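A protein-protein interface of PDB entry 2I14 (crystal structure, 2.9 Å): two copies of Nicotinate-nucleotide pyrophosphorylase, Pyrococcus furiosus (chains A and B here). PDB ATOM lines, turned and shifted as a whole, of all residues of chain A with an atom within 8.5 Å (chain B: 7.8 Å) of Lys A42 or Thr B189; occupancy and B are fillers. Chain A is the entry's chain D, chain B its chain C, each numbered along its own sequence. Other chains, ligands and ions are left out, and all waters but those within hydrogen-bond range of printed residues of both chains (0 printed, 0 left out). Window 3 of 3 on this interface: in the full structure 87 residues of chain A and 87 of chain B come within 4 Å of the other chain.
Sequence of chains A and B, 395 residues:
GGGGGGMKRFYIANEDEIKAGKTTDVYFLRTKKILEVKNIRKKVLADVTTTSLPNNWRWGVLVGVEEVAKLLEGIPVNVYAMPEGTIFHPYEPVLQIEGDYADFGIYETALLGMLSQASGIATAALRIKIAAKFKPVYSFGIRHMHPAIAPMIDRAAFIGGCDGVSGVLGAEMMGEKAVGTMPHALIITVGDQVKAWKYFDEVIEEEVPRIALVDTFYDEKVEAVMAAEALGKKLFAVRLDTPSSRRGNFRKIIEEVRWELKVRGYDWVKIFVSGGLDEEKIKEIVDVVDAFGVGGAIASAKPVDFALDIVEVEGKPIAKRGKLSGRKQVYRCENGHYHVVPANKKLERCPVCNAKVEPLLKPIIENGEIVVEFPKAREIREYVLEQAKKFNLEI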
ATOM      1  N   THR A  31      -8.796 -18.892 -16.034  1.00  0.00           N
ATOM      2  CA  THR A  31      -9.254 -20.229 -15.681  1.00  0.00           C
ATOM      3  C   THR A  31     -10.205 -20.737 -16.756  1.00  0.00           C
ATOM      4  O   THR A  31     -10.259 -21.935 -17.036  1.00  0.00           O
ATOM      5  CB  THR A  31      -9.973 -20.246 -14.326  1.00  0.00           C
ATOM      6  OG1 THR A  31      -9.008 -20.080 -13.291  1.00  0.00           O
ATOM      7  CG2 THR A  31     -10.694 -21.562 -14.107  1.00  0.00           C
ATOM      8  N   ILE A  34      -7.770 -21.876 -19.839  1.00  0.00           N
ATOM      9  CA  ILE A  34      -7.204 -23.205 -19.621  1.00  0.00           C
ATOM     10  C   ILE A  34      -8.250 -24.291 -19.878  1.00  0.00           C
ATOM     11  O   ILE A  34      -8.011 -25.224 -20.644  1.00  0.00           O
ATOM     12  CB  ILE A  34      -6.707 -23.396 -18.158  1.00  0.00           C
ATOM     13  CG1 ILE A  34      -5.784 -22.248 -17.742  1.00  0.00           C
ATOM     14  CG2 ILE A  34      -6.000 -24.748 -18.023  1.00  0.00           C
ATOM     15  CD1 ILE A  34      -4.476 -22.207 -18.474  1.00  0.00           C
ATOM     16  N   LEU A  35      -9.400 -24.158 -19.220  1.00  0.00           N
ATOM     17  CA  LEU A  35     -10.503 -25.109 -19.327  1.00  0.00           C
ATOM     18  C   LEU A  35     -11.102 -25.221 -20.714  1.00  0.00           C
ATOM     19  O   LEU A  35     -11.387 -26.316 -21.188  1.00  0.00           O
ATOM     20  CB  LEU A  35     -11.619 -24.719 -18.365  1.00  0.00           C
ATOM     21  CG  LEU A  35     -11.356 -24.842 -16.874  1.00  0.00           C
ATOM     22  CD1 LEU A  35     -12.502 -24.195 -16.106  1.00  0.00           C
ATOM     23  CD2 LEU A  35     -11.197 -26.316 -16.509  1.00  0.00           C
ATOM     24  N   ASN A  39      -9.753 -27.769 -23.320  1.00  0.00           N
ATOM     25  CA  ASN A  39     -11.106 -28.319 -23.238  1.00  0.00           C
ATOM     26  C   ASN A  39     -11.345 -29.307 -22.095  1.00  0.00           C
ATOM     27  O   ASN A  39     -11.313 -30.521 -22.284  1.00  0.00           O
ATOM     28  CB  ASN A  39     -11.498 -28.965 -24.570  1.00  0.00           C
ATOM     29  CG  ASN A  39     -12.953 -28.713 -24.929  1.00  0.00           C
ATOM     30  OD1 ASN A  39     -13.480 -29.288 -25.882  1.00  0.00           O
ATOM     31  ND2 ASN A  39     -13.607 -27.839 -24.166  1.00  0.00           N
ATOM     32  N   ILE A  40     -11.598 -28.766 -20.907  1.00  0.00           N
ATOM     33  CA  ILE A  40     -11.849 -29.575 -19.724  1.00  0.00           C
ATOM     34  C   ILE A  40     -13.240 -29.227 -19.214  1.00  0.00           C
ATOM     35  O   ILE A  40     -13.396 -28.659 -18.131  1.00  0.00           O
ATOM     36  CB  ILE A  40     -10.810 -29.276 -18.620  1.00  0.00           C
ATOM     37  CG1 ILE A  40      -9.399 -29.437 -19.185  1.00  0.00           C
ATOM     38  CG2 ILE A  40     -11.013 -30.215 -17.428  1.00  0.00           C
ATOM     39  CD1 ILE A  40      -8.304 -28.987 -18.237  1.00  0.00           C
ATOM     40  N   ARG A  41     -14.251 -29.564 -20.002  1.00  0.00           N
ATOM     41  CA  ARG A  41     -15.619 -29.270 -19.621  1.00  0.00           C
ATOM     42  C   ARG A  41     -16.161 -30.371 -18.713  1.00  0.00           C
ATOM     43  O   ARG A  41     -15.965 -31.556 -18.977  1.00  0.00           O
ATOM     44  CB  ARG A  41     -16.493 -29.153 -20.872  1.00  0.00           C
ATOM     45  CG  ARG A  41     -15.828 -28.426 -22.035  1.00  0.00           C
ATOM     46  CD  ARG A  41     -15.656 -26.931 -21.797  1.00  0.00           C
ATOM     47  NE  ARG A  41     -16.942 -26.241 -21.702  1.00  0.00           N
ATOM     48  CZ  ARG A  41     -17.093 -24.924 -21.812  1.00  0.00           C
ATOM     49  NH1 ARG A  41     -16.036 -24.148 -22.025  1.00  0.00           N
ATOM     50  NH2 ARG A  41     -18.301 -24.384 -21.704  1.00  0.00           N
ATOM     51  N   LYS A  42     -16.827 -29.967 -17.636  1.00  0.00           N
ATOM     52  CA  LYS A  42     -17.423 -30.915 -16.703  1.00  0.00           C
ATOM     53  C   LYS A  42     -18.371 -30.256 -15.692  1.00  0.00           C
ATOM     54  O   LYS A  42     -18.201 -29.091 -15.318  1.00  0.00           O
ATOM     55  CB  LYS A  42     -16.336 -31.704 -15.971  1.00  0.00           C
ATOM     56  CG  LYS A  42     -15.304 -30.864 -15.270  1.00  0.00           C
ATOM     57  CD  LYS A  42     -14.448 -31.727 -14.350  1.00  0.00           C
ATOM     58  CE  LYS A  42     -13.687 -32.796 -15.113  1.00  0.00           C
ATOM     59  NZ  LYS A  42     -12.933 -33.673 -14.178  1.00  0.00           N
ATOM     60  N   LYS A  43     -19.376 -31.021 -15.271  1.00  0.00           N
ATOM     61  CA  LYS A  43     -20.382 -30.560 -14.323  1.00  0.00           C
ATOM     62  C   LYS A  43     -19.854 -30.559 -12.889  1.00  0.00           C
ATOM     63  O   LYS A  43     -19.259 -31.536 -12.425  1.00  0.00           O
ATOM     64  CB  LYS A  43     -21.632 -31.455 -14.412  1.00  0.00           C
ATOM     65  CG  LYS A  43     -22.920 -30.789 -14.939  1.00  0.00           C
ATOM     66  CD  LYS A  43     -22.810 -30.306 -16.396  1.00  0.00           C
ATOM     67  CE  LYS A  43     -24.186 -30.227 -17.095  1.00  0.00           C
ATOM     68  NZ  LYS A  43     -25.203 -29.336 -16.448  1.00  0.00           N
ATOM     69  N   VAL A  44     -20.084 -29.445 -12.197  1.00  0.00           N
ATOM     70  CA  VAL A  44     -19.662 -29.283 -10.814  1.00  0.00           C
ATOM     71  C   VAL A  44     -20.745 -28.585  -9.999  1.00  0.00           C
ATOM     72  O   VAL A  44     -21.584 -27.851 -10.534  1.00  0.00           O
ATOM     73  CB  VAL A  44     -18.370 -28.438 -10.710  1.00  0.00           C
ATOM     74  CG1 VAL A  44     -17.210 -29.182 -11.327  1.00  0.00           C
ATOM     75  CG2 VAL A  44     -18.566 -27.090 -11.395  1.00  0.00           C
ATOM     76  N   LEU A  45     -20.729 -28.835  -8.698  1.00  0.00           N
ATOM     77  CA  LEU A  45     -21.666 -28.196  -7.795  1.00  0.00           C
ATOM     78  C   LEU A  45     -20.825 -27.345  -6.848  1.00  0.00           C
ATOM     79  O   LEU A  45     -19.965 -27.867  -6.132  1.00  0.00           O
ATOM     80  CB  LEU A  45     -22.459 -29.234  -6.995  1.00  0.00           C
ATOM     81  CG  LEU A  45     -23.496 -28.668  -6.016  1.00  0.00           C
ATOM     82  CD1 LEU A  45     -24.452 -27.733  -6.747  1.00  0.00           C
ATOM     83  CD2 LEU A  45     -24.260 -29.800  -5.362  1.00  0.00           C
ATOM     84  N   GLU A  98     -24.941 -25.236 -10.008  1.00  0.00           N
ATOM     85  CA  GLU A  98     -24.561 -26.448 -10.701  1.00  0.00           C
ATOM     86  C   GLU A  98     -24.334 -26.189 -12.179  1.00  0.00           C
ATOM     87  O   GLU A  98     -25.084 -25.445 -12.816  1.00  0.00           O
ATOM     88  CB  GLU A  98     -25.640 -27.497 -10.514  1.00  0.00           C
ATOM     89  CG  GLU A  98     -25.141 -28.888 -10.744  1.00  0.00           C
ATOM     90  CD  GLU A  98     -26.072 -29.930 -10.164  1.00  0.00           C
ATOM     91  OE1 GLU A  98     -25.700 -31.128 -10.204  1.00  0.00           O
ATOM     92  OE2 GLU A  98     -27.164 -29.550  -9.668  1.00  0.00           O
ATOM     93  N   GLY A  99     -23.287 -26.797 -12.720  1.00  0.00           N
ATOM     94  CA  GLY A  99     -22.992 -26.606 -14.122  1.00  0.00           C
ATOM     95  C   GLY A  99     -21.521 -26.706 -14.444  1.00  0.00           C
ATOM     96  O   GLY A  99     -20.718 -27.129 -13.616  1.00  0.00           O
ATOM     97  N   ASP A 100     -21.172 -26.320 -15.664  1.00  0.00           N
ATOM     98  CA  ASP A 100     -19.789 -26.355 -16.112  1.00  0.00           C
ATOM     99  C   ASP A 100     -19.107 -25.143 -15.495  1.00  0.00           C
ATOM    100  O   ASP A 100     -19.493 -24.008 -15.778  1.00  0.00           O
ATOM    101  CB  ASP A 100     -19.740 -26.260 -17.644  1.00  0.00           C
ATOM    102  CG  ASP A 100     -18.373 -26.616 -18.223  1.00  0.00           C
ATOM    103  OD1 ASP A 100     -18.219 -26.523 -19.463  1.00  0.00           O
ATOM    104  OD2 ASP A 100     -17.465 -26.991 -17.446  1.00  0.00           O
ATOM    105  N   TYR A 101     -18.107 -25.372 -14.649  1.00  0.00           N
ATOM    106  CA  TYR A 101     -17.422 -24.256 -14.025  1.00  0.00           C
ATOM    107  C   TYR A 101     -17.002 -23.266 -15.096  1.00  0.00           C
ATOM    108  O   TYR A 101     -16.992 -22.052 -14.875  1.00  0.00           O
ATOM    109  CB  TYR A 101     -16.171 -24.707 -13.263  1.00  0.00           C
ATOM    110  CG  TYR A 101     -15.503 -23.538 -12.565  1.00  0.00           C
ATOM    111  CD1 TYR A 101     -16.064 -22.984 -11.414  1.00  0.00           C
ATOM    112  CD2 TYR A 101     -14.376 -22.917 -13.119  1.00  0.00           C
ATOM    113  CE1 TYR A 101     -15.531 -21.842 -10.838  1.00  0.00           C
ATOM    114  CE2 TYR A 101     -13.833 -21.769 -12.549  1.00  0.00           C
ATOM    115  CZ  TYR A 101     -14.418 -21.235 -11.410  1.00  0.00           C
ATOM    116  OH  TYR A 101     -13.914 -20.086 -10.835  1.00  0.00           O
ATOM    117  N   ALA A 102     -16.653 -23.796 -16.262  1.00  0.00           N
ATOM    118  CA  ALA A 102     -16.212 -22.968 -17.374  1.00  0.00           C
ATOM    119  C   ALA A 102     -17.234 -21.897 -17.740  1.00  0.00           C
ATOM    120  O   ALA A 102     -16.883 -20.860 -18.305  1.00  0.00           O
ATOM    121  CB  ALA A 102     -15.921 -23.839 -18.576  1.00  0.00           C
ATOM    122  N   ASP A 103     -18.495 -22.139 -17.399  1.00  0.00           N
ATOM    123  CA  ASP A 103     -19.571 -21.199 -17.723  1.00  0.00           C
ATOM    124  C   ASP A 103     -19.819 -20.073 -16.710  1.00  0.00           C
ATOM    125  O   ASP A 103     -19.805 -18.900 -17.074  1.00  0.00           O
ATOM    126  CB  ASP A 103     -20.884 -21.974 -17.955  1.00  0.00           C
ATOM    127  CG  ASP A 103     -20.876 -22.806 -19.255  1.00  0.00           C
ATOM    128  OD1 ASP A 103     -21.654 -23.792 -19.331  1.00  0.00           O
ATOM    129  OD2 ASP A 103     -20.115 -22.472 -20.201  1.00  0.00           O
ATOM    130  N   PHE A 104     -20.035 -20.424 -15.445  1.00  0.00           N
ATOM    131  CA  PHE A 104     -20.326 -19.434 -14.405  1.00  0.00           C
ATOM    132  C   PHE A 104     -19.138 -18.951 -13.564  1.00  0.00           C
ATOM    133  O   PHE A 104     -19.188 -17.864 -12.979  1.00  0.00           O
ATOM    134  CB  PHE A 104     -21.401 -19.990 -13.473  1.00  0.00           C
ATOM    135  CG  PHE A 104     -20.943 -21.161 -12.653  1.00  0.00           C
ATOM    136  CD1 PHE A 104     -20.345 -20.972 -11.413  1.00  0.00           C
ATOM    137  CD2 PHE A 104     -21.096 -22.456 -13.122  1.00  0.00           C
ATOM    138  CE1 PHE A 104     -19.908 -22.054 -10.657  1.00  0.00           C
ATOM    139  CE2 PHE A 104     -20.659 -23.549 -12.368  1.00  0.00           C
ATOM    140  CZ  PHE A 104     -20.067 -23.345 -11.136  1.00  0.00           C
ATOM    141  N   ILE A 310     -16.315 -25.330  -4.951  1.00  0.00           N
ATOM    142  CA  ILE A 310     -16.852 -26.565  -5.529  1.00  0.00           C
ATOM    143  C   ILE A 310     -16.726 -27.704  -4.507  1.00  0.00           C
ATOM    144  O   ILE A 310     -15.629 -28.053  -4.065  1.00  0.00           O
ATOM    145  CB  ILE A 310     -16.131 -26.921  -6.854  1.00  0.00           C
ATOM    146  CG1 ILE A 310     -14.661 -26.535  -6.771  1.00  0.00           C
ATOM    147  CG2 ILE A 310     -16.759 -26.153  -8.011  1.00  0.00           C
ATOM    148  CD1 ILE A 310     -13.963 -26.542  -8.118  1.00  0.00           C
ATOM    149  N   GLU A 312     -18.500 -30.641  -5.088  1.00  0.00           N
ATOM    150  CA  GLU A 312     -18.814 -31.859  -5.827  1.00  0.00           C
ATOM    151  C   GLU A 312     -18.559 -31.670  -7.325  1.00  0.00           C
ATOM    152  O   GLU A 312     -18.956 -30.657  -7.916  1.00  0.00           O
ATOM    153  CB  GLU A 312     -20.272 -32.264  -5.589  1.00  0.00           C
ATOM    154  CG  GLU A 312     -20.554 -33.737  -5.855  1.00  0.00           C
ATOM    155  CD  GLU A 312     -21.983 -34.132  -5.515  1.00  0.00           C
ATOM    156  OE1 GLU A 312     -22.914 -33.621  -6.180  1.00  0.00           O
ATOM    157  OE2 GLU A 312     -22.170 -34.954  -4.582  1.00  0.00           O
ATOM    158  N   VAL A 313     -17.886 -32.649  -7.929  1.00  0.00           N
ATOM    159  CA  VAL A 313     -17.570 -32.610  -9.352  1.00  0.00           C
ATOM    160  C   VAL A 313     -18.010 -33.925  -9.995  1.00  0.00           C
ATOM    161  O   VAL A 313     -17.457 -34.990  -9.693  1.00  0.00           O
ATOM    162  CB  VAL A 313     -16.060 -32.433  -9.582  1.00  0.00           C
ATOM    163  CG1 VAL A 313     -15.781 -32.191 -11.045  1.00  0.00           C
ATOM    164  CG2 VAL A 313     -15.540 -31.284  -8.747  1.00  0.00           C
ATOM    165  N   GLU A 314     -19.007 -33.847 -10.874  1.00  0.00           N
ATOM    166  CA  GLU A 314     -19.537 -35.022 -11.563  1.00  0.00           C
ATOM    167  C   GLU A 314     -20.091 -36.041 -10.575  1.00  0.00           C
ATOM    168  O   GLU A 314     -19.728 -37.217 -10.615  1.00  0.00           O
ATOM    169  CB  GLU A 314     -18.450 -35.686 -12.413  1.00  0.00           C
ATOM    170  CG  GLU A 314     -18.779 -35.768 -13.899  1.00  0.00           C
ATOM    171  CD  GLU A 314     -17.907 -34.849 -14.751  1.00  0.00           C
ATOM    172  OE1 GLU A 314     -16.673 -35.068 -14.798  1.00  0.00           O
ATOM    173  OE2 GLU A 314     -18.460 -33.910 -15.372  1.00  0.00           O
ATOM    174  N   GLY A 315     -20.964 -35.582  -9.688  1.00  0.00           N
ATOM    175  CA  GLY A 315     -21.559 -36.473  -8.706  1.00  0.00           C
ATOM    176  C   GLY A 315     -20.570 -37.037  -7.704  1.00  0.00           C
ATOM    177  O   GLY A 315     -20.932 -37.864  -6.864  1.00  0.00           O
ATOM    178  N   LYS A 316     -19.321 -36.591  -7.793  1.00  0.00           N
ATOM    179  CA  LYS A 316     -18.269 -37.041  -6.887  1.00  0.00           C
ATOM    180  C   LYS A 316     -17.981 -35.972  -5.829  1.00  0.00           C
ATOM    181  O   LYS A 316     -17.734 -34.808  -6.161  1.00  0.00           O
ATOM    182  CB  LYS A 316     -16.992 -37.331  -7.672  1.00  0.00           C
ATOM    183  CG  LYS A 316     -17.140 -38.418  -8.722  1.00  0.00           C
ATOM    184  CD  LYS A 316     -17.321 -39.787  -8.082  1.00  0.00           C
ATOM    185  CE  LYS A 316     -17.266 -40.899  -9.128  1.00  0.00           C
ATOM    186  NZ  LYS A 316     -17.230 -42.254  -8.504  1.00  0.00           N
ATOM    187  N   ILE A 318     -16.011 -33.781  -3.566  1.00  0.00           N
ATOM    188  CA  ILE A 318     -14.648 -33.267  -3.473  1.00  0.00           C
ATOM    189  C   ILE A 318     -14.586 -31.756  -3.265  1.00  0.00           C
ATOM    190  O   ILE A 318     -15.204 -30.994  -4.002  1.00  0.00           O
ATOM    191  CB  ILE A 318     -13.829 -33.641  -4.729  1.00  0.00           C
ATOM    192  CG1 ILE A 318     -13.315 -35.074  -4.580  1.00  0.00           C
ATOM    193  CG2 ILE A 318     -12.666 -32.671  -4.931  1.00  0.00           C
ATOM    194  CD1 ILE A 318     -12.464 -35.567  -5.735  1.00  0.00           C
ATOM    195  N   PRO B 183      -6.867 -20.065  -9.277  1.00  0.00           N
ATOM    196  CA  PRO B 183      -7.991 -20.323  -8.379  1.00  0.00           C
ATOM    197  C   PRO B 183      -7.916 -21.761  -7.907  1.00  0.00           C
ATOM    198  O   PRO B 183      -7.180 -22.558  -8.473  1.00  0.00           O
ATOM    199  CB  PRO B 183      -9.211 -20.092  -9.268  1.00  0.00           C
ATOM    200  CG  PRO B 183      -8.712 -19.209 -10.338  1.00  0.00           C
ATOM    201  CD  PRO B 183      -7.366 -19.817 -10.634  1.00  0.00           C
ATOM    202  N   HIS B 184      -8.675 -22.085  -6.868  1.00  0.00           N
ATOM    203  CA  HIS B 184      -8.722 -23.442  -6.348  1.00  0.00           C
ATOM    204  C   HIS B 184      -9.612 -24.254  -7.266  1.00  0.00           C
ATOM    205  O   HIS B 184      -9.467 -25.472  -7.390  1.00  0.00           O
ATOM    206  CB  HIS B 184      -9.325 -23.450  -4.949  1.00  0.00           C
ATOM    207  CG  HIS B 184      -8.310 -23.372  -3.863  1.00  0.00           C
ATOM    208  ND1 HIS B 184      -7.596 -24.470  -3.444  1.00  0.00           N
ATOM    209  CD2 HIS B 184      -7.851 -22.321  -3.145  1.00  0.00           C
ATOM    210  CE1 HIS B 184      -6.736 -24.100  -2.513  1.00  0.00           C
ATOM    211  NE2 HIS B 184      -6.869 -22.801  -2.314  1.00  0.00           N
ATOM    212  N   ALA B 185     -10.553 -23.558  -7.895  1.00  0.00           N
ATOM    213  CA  ALA B 185     -11.492 -24.194  -8.803  1.00  0.00           C
ATOM    214  C   ALA B 185     -10.730 -24.838  -9.952  1.00  0.00           C
ATOM    215  O   ALA B 185     -10.990 -25.990 -10.306  1.00  0.00           O
ATOM    216  CB  ALA B 185     -12.491 -23.164  -9.335  1.00  0.00           C
ATOM    217  N   LEU B 186      -9.782 -24.098 -10.525  1.00  0.00           N
ATOM    218  CA  LEU B 186      -9.001 -24.623 -11.635  1.00  0.00           C
ATOM    219  C   LEU B 186      -8.392 -25.965 -11.288  1.00  0.00           C
ATOM    220  O   LEU B 186      -8.638 -26.957 -11.952  1.00  0.00           O
ATOM    221  CB  LEU B 186      -7.894 -23.646 -12.029  1.00  0.00           C
ATOM    222  CG  LEU B 186      -6.985 -24.154 -13.148  1.00  0.00           C
ATOM    223  CD1 LEU B 186      -6.420 -22.979 -13.926  1.00  0.00           C
ATOM    224  CD2 LEU B 186      -5.877 -25.004 -12.554  1.00  0.00           C
ATOM    225  N   ILE B 187      -7.595 -26.000 -10.240  1.00  0.00           N
ATOM    226  CA  ILE B 187      -6.961 -27.239  -9.842  1.00  0.00           C
ATOM    227  C   ILE B 187      -7.947 -28.350  -9.512  1.00  0.00           C
ATOM    228  O   ILE B 187      -7.694 -29.507  -9.827  1.00  0.00           O
ATOM    229  CB  ILE B 187      -6.046 -26.991  -8.644  1.00  0.00           C
ATOM    230  CG1 ILE B 187      -4.978 -25.973  -9.053  1.00  0.00           C
ATOM    231  CG2 ILE B 187      -5.437 -28.303  -8.161  1.00  0.00           C
ATOM    232  CD1 ILE B 187      -4.170 -25.432  -7.910  1.00  0.00           C
ATOM    233  N   ILE B 188      -9.077 -28.010  -8.895  1.00  0.00           N
ATOM    234  CA  ILE B 188     -10.065 -29.031  -8.530  1.00  0.00           C
ATOM    235  C   ILE B 188     -10.860 -29.598  -9.708  1.00  0.00           C
ATOM    236  O   ILE B 188     -11.120 -30.800  -9.750  1.00  0.00           O
ATOM    237  CB  ILE B 188     -11.060 -28.519  -7.456  1.00  0.00           C
ATOM    238  CG1 ILE B 188     -10.309 -28.187  -6.158  1.00  0.00           C
ATOM    239  CG2 ILE B 188     -12.111 -29.592  -7.175  1.00  0.00           C
ATOM    240  CD1 ILE B 188     -11.208 -27.788  -4.985  1.00  0.00           C
ATOM    241  N   THR B 189     -11.250 -28.755 -10.662  1.00  0.00           N
ATOM    242  CA  THR B 189     -12.008 -29.260 -11.806  1.00  0.00           C
ATOM    243  C   THR B 189     -11.073 -30.086 -12.680  1.00  0.00           C
ATOM    244  O   THR B 189     -11.452 -31.160 -13.149  1.00  0.00           O
ATOM    245  CB  THR B 189     -12.643 -28.130 -12.668  1.00  0.00           C
ATOM    246  OG1 THR B 189     -11.628 -27.484 -13.442  1.00  0.00           O
ATOM    247  CG2 THR B 189     -13.350 -27.102 -11.785  1.00  0.00           C
ATOM    248  N   VAL B 190      -9.853 -29.589 -12.888  1.00  0.00           N
ATOM    249  CA  VAL B 190      -8.849 -30.298 -13.685  1.00  0.00           C
ATOM    250  C   VAL B 190      -8.527 -31.634 -13.016  1.00  0.00           C
ATOM    251  O   VAL B 190      -8.012 -32.547 -13.655  1.00  0.00           O
ATOM    252  CB  VAL B 190      -7.549 -29.475 -13.824  1.00  0.00           C
ATOM    253  CG1 VAL B 190      -6.440 -30.341 -14.388  1.00  0.00           C
ATOM    254  CG2 VAL B 190      -7.787 -28.277 -14.736  1.00  0.00           C
ATOM    255  N   GLY B 191      -8.831 -31.732 -11.723  1.00  0.00           N
ATOM    256  CA  GLY B 191      -8.612 -32.965 -10.982  1.00  0.00           C
ATOM    257  C   GLY B 191      -7.202 -33.334 -10.547  1.00  0.00           C
ATOM    258  O   GLY B 191      -7.006 -34.360  -9.893  1.00  0.00           O
ATOM    259  N   ASP B 192      -6.214 -32.517 -10.897  1.00  0.00           N
ATOM    260  CA  ASP B 192      -4.847 -32.813 -10.510  1.00  0.00           C
ATOM    261  C   ASP B 192      -3.992 -31.564 -10.404  1.00  0.00           C
ATOM    262  O   ASP B 192      -3.936 -30.763 -11.330  1.00  0.00           O
ATOM    263  CB  ASP B 192      -4.229 -33.768 -11.518  1.00  0.00           C
ATOM    264  CG  ASP B 192      -2.817 -34.148 -11.161  1.00  0.00           C
ATOM    265  OD1 ASP B 192      -1.909 -33.289 -11.292  1.00  0.00           O
ATOM    266  OD2 ASP B 192      -2.622 -35.309 -10.737  1.00  0.00           O
ATOM    267  N   ALA B 196      -2.848 -29.359 -13.580  1.00  0.00           N
ATOM    268  CA  ALA B 196      -3.425 -28.020 -13.541  1.00  0.00           C
ATOM    269  C   ALA B 196      -2.418 -26.918 -13.856  1.00  0.00           C
ATOM    270  O   ALA B 196      -2.572 -26.192 -14.844  1.00  0.00           O
ATOM    271  CB  ALA B 196      -4.056 -27.772 -12.170  1.00  0.00           C
ATOM    272  N   PHE B 217      -5.052 -30.109  -1.561  1.00  0.00           N
ATOM    273  CA  PHE B 217      -5.411 -31.416  -1.010  1.00  0.00           C
ATOM    274  C   PHE B 217      -4.291 -31.875  -0.084  1.00  0.00           C
ATOM    275  O   PHE B 217      -4.527 -32.341   1.033  1.00  0.00           O
ATOM    276  CB  PHE B 217      -5.577 -32.454  -2.132  1.00  0.00           C
ATOM    277  CG  PHE B 217      -6.593 -32.079  -3.175  1.00  0.00           C
ATOM    278  CD1 PHE B 217      -7.925 -31.873  -2.829  1.00  0.00           C
ATOM    279  CD2 PHE B 217      -6.217 -31.943  -4.508  1.00  0.00           C
ATOM    280  CE1 PHE B 217      -8.869 -31.538  -3.796  1.00  0.00           C
ATOM    281  CE2 PHE B 217      -7.148 -31.610  -5.484  1.00  0.00           C
ATOM    282  CZ  PHE B 217      -8.481 -31.406  -5.128  1.00  0.00           C
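The backbone carbonyl oxygen (O) of Thr B189 lies within hydrogen-bond range of the side-chain amino group (NZ) of Lys A42 (3.1 Å).
The backbone NH (N) of Glu A312 is in hydrogen-bond range of the backbone carbonyl oxygen (O) of Ile A318 (3.5 Å).
The backbone NH (N) of Lys A42 is in hydrogen-bond range of the side-chain carboxylate (OD2) of Asp A100 (3.0 Å).
The backbone carbonyl oxygen (O) of Leu A35 sits at hydrogen-bond distance from the backbone NH (N) of Ile A40, 2.5 Å away.
O of Leu B186 sits at hydrogen-bond distance from OG1 of Thr B189, at 3.4 Å.
Thr A31 touches Pro B183.
Leu B186 touches Thr A31.
Leu B186 touches Ile A34 (CD1 to CG1, 3.9 Å).
CD2 of Leu A35 touches OG1 of Thr B189 (3.3 Å).
Ile A40 touches Val B190 (CD1 to CG2, 3.6 Å).
CB of Tyr A101 touches CG2 of Thr B189, at 3.98 Å.
Ile A310 touches Ala B185.
Ile B188 touches Ile A310.
CG2 of Thr B189 touches CD1 of Ile A310 (3.8 Å).
Ile A318 touches Ile B188 (CG2 to CG2, 3.9 Å).
Printed residues of chain A within 4 Å of Ile B188: Ile A310 and Ile A318.
Printed residues of chain B within 4 Å of Tyr A101: Ala B185 (3.4 Å) and Thr B189 (3.98 Å).
Printed residues of chain B within 4 Å of Thr A31: Pro B183 and Leu B186.
Of the printed residues of chain B, Ile A40 touches Val B190 (3.6 Å).
The nearest residue of chain B that does not touch Lys A42 is Val B190 (5.0 Å).
The nearest printed residue of chain A that does not touch Thr B189 is Ile A40 (4.4 Å).
The nearest printed residue of chain B that does not touch Thr A31 is Ala B185 (5.3 Å).
Of the 24 printed residues of chain A, 8 touch a printed residue of chain B.
Hydrophobic or aromatic side chains of chain A within 4 Å of the printed part of chain B: Ile A34, Leu A35, Ile A40, Tyr A101, Ile A310 and Ile A318.
Hydrophobic or aromatic side chains of chain B within 4 Å of the printed part of chain A: Pro B183, Ala B185, Leu B186, Ile B188 and Val B190.
No position is printed for both chains.
Of the 12 pairs that touch across the chains among the printed residues, none has its exchanged pair printed and touching as well.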
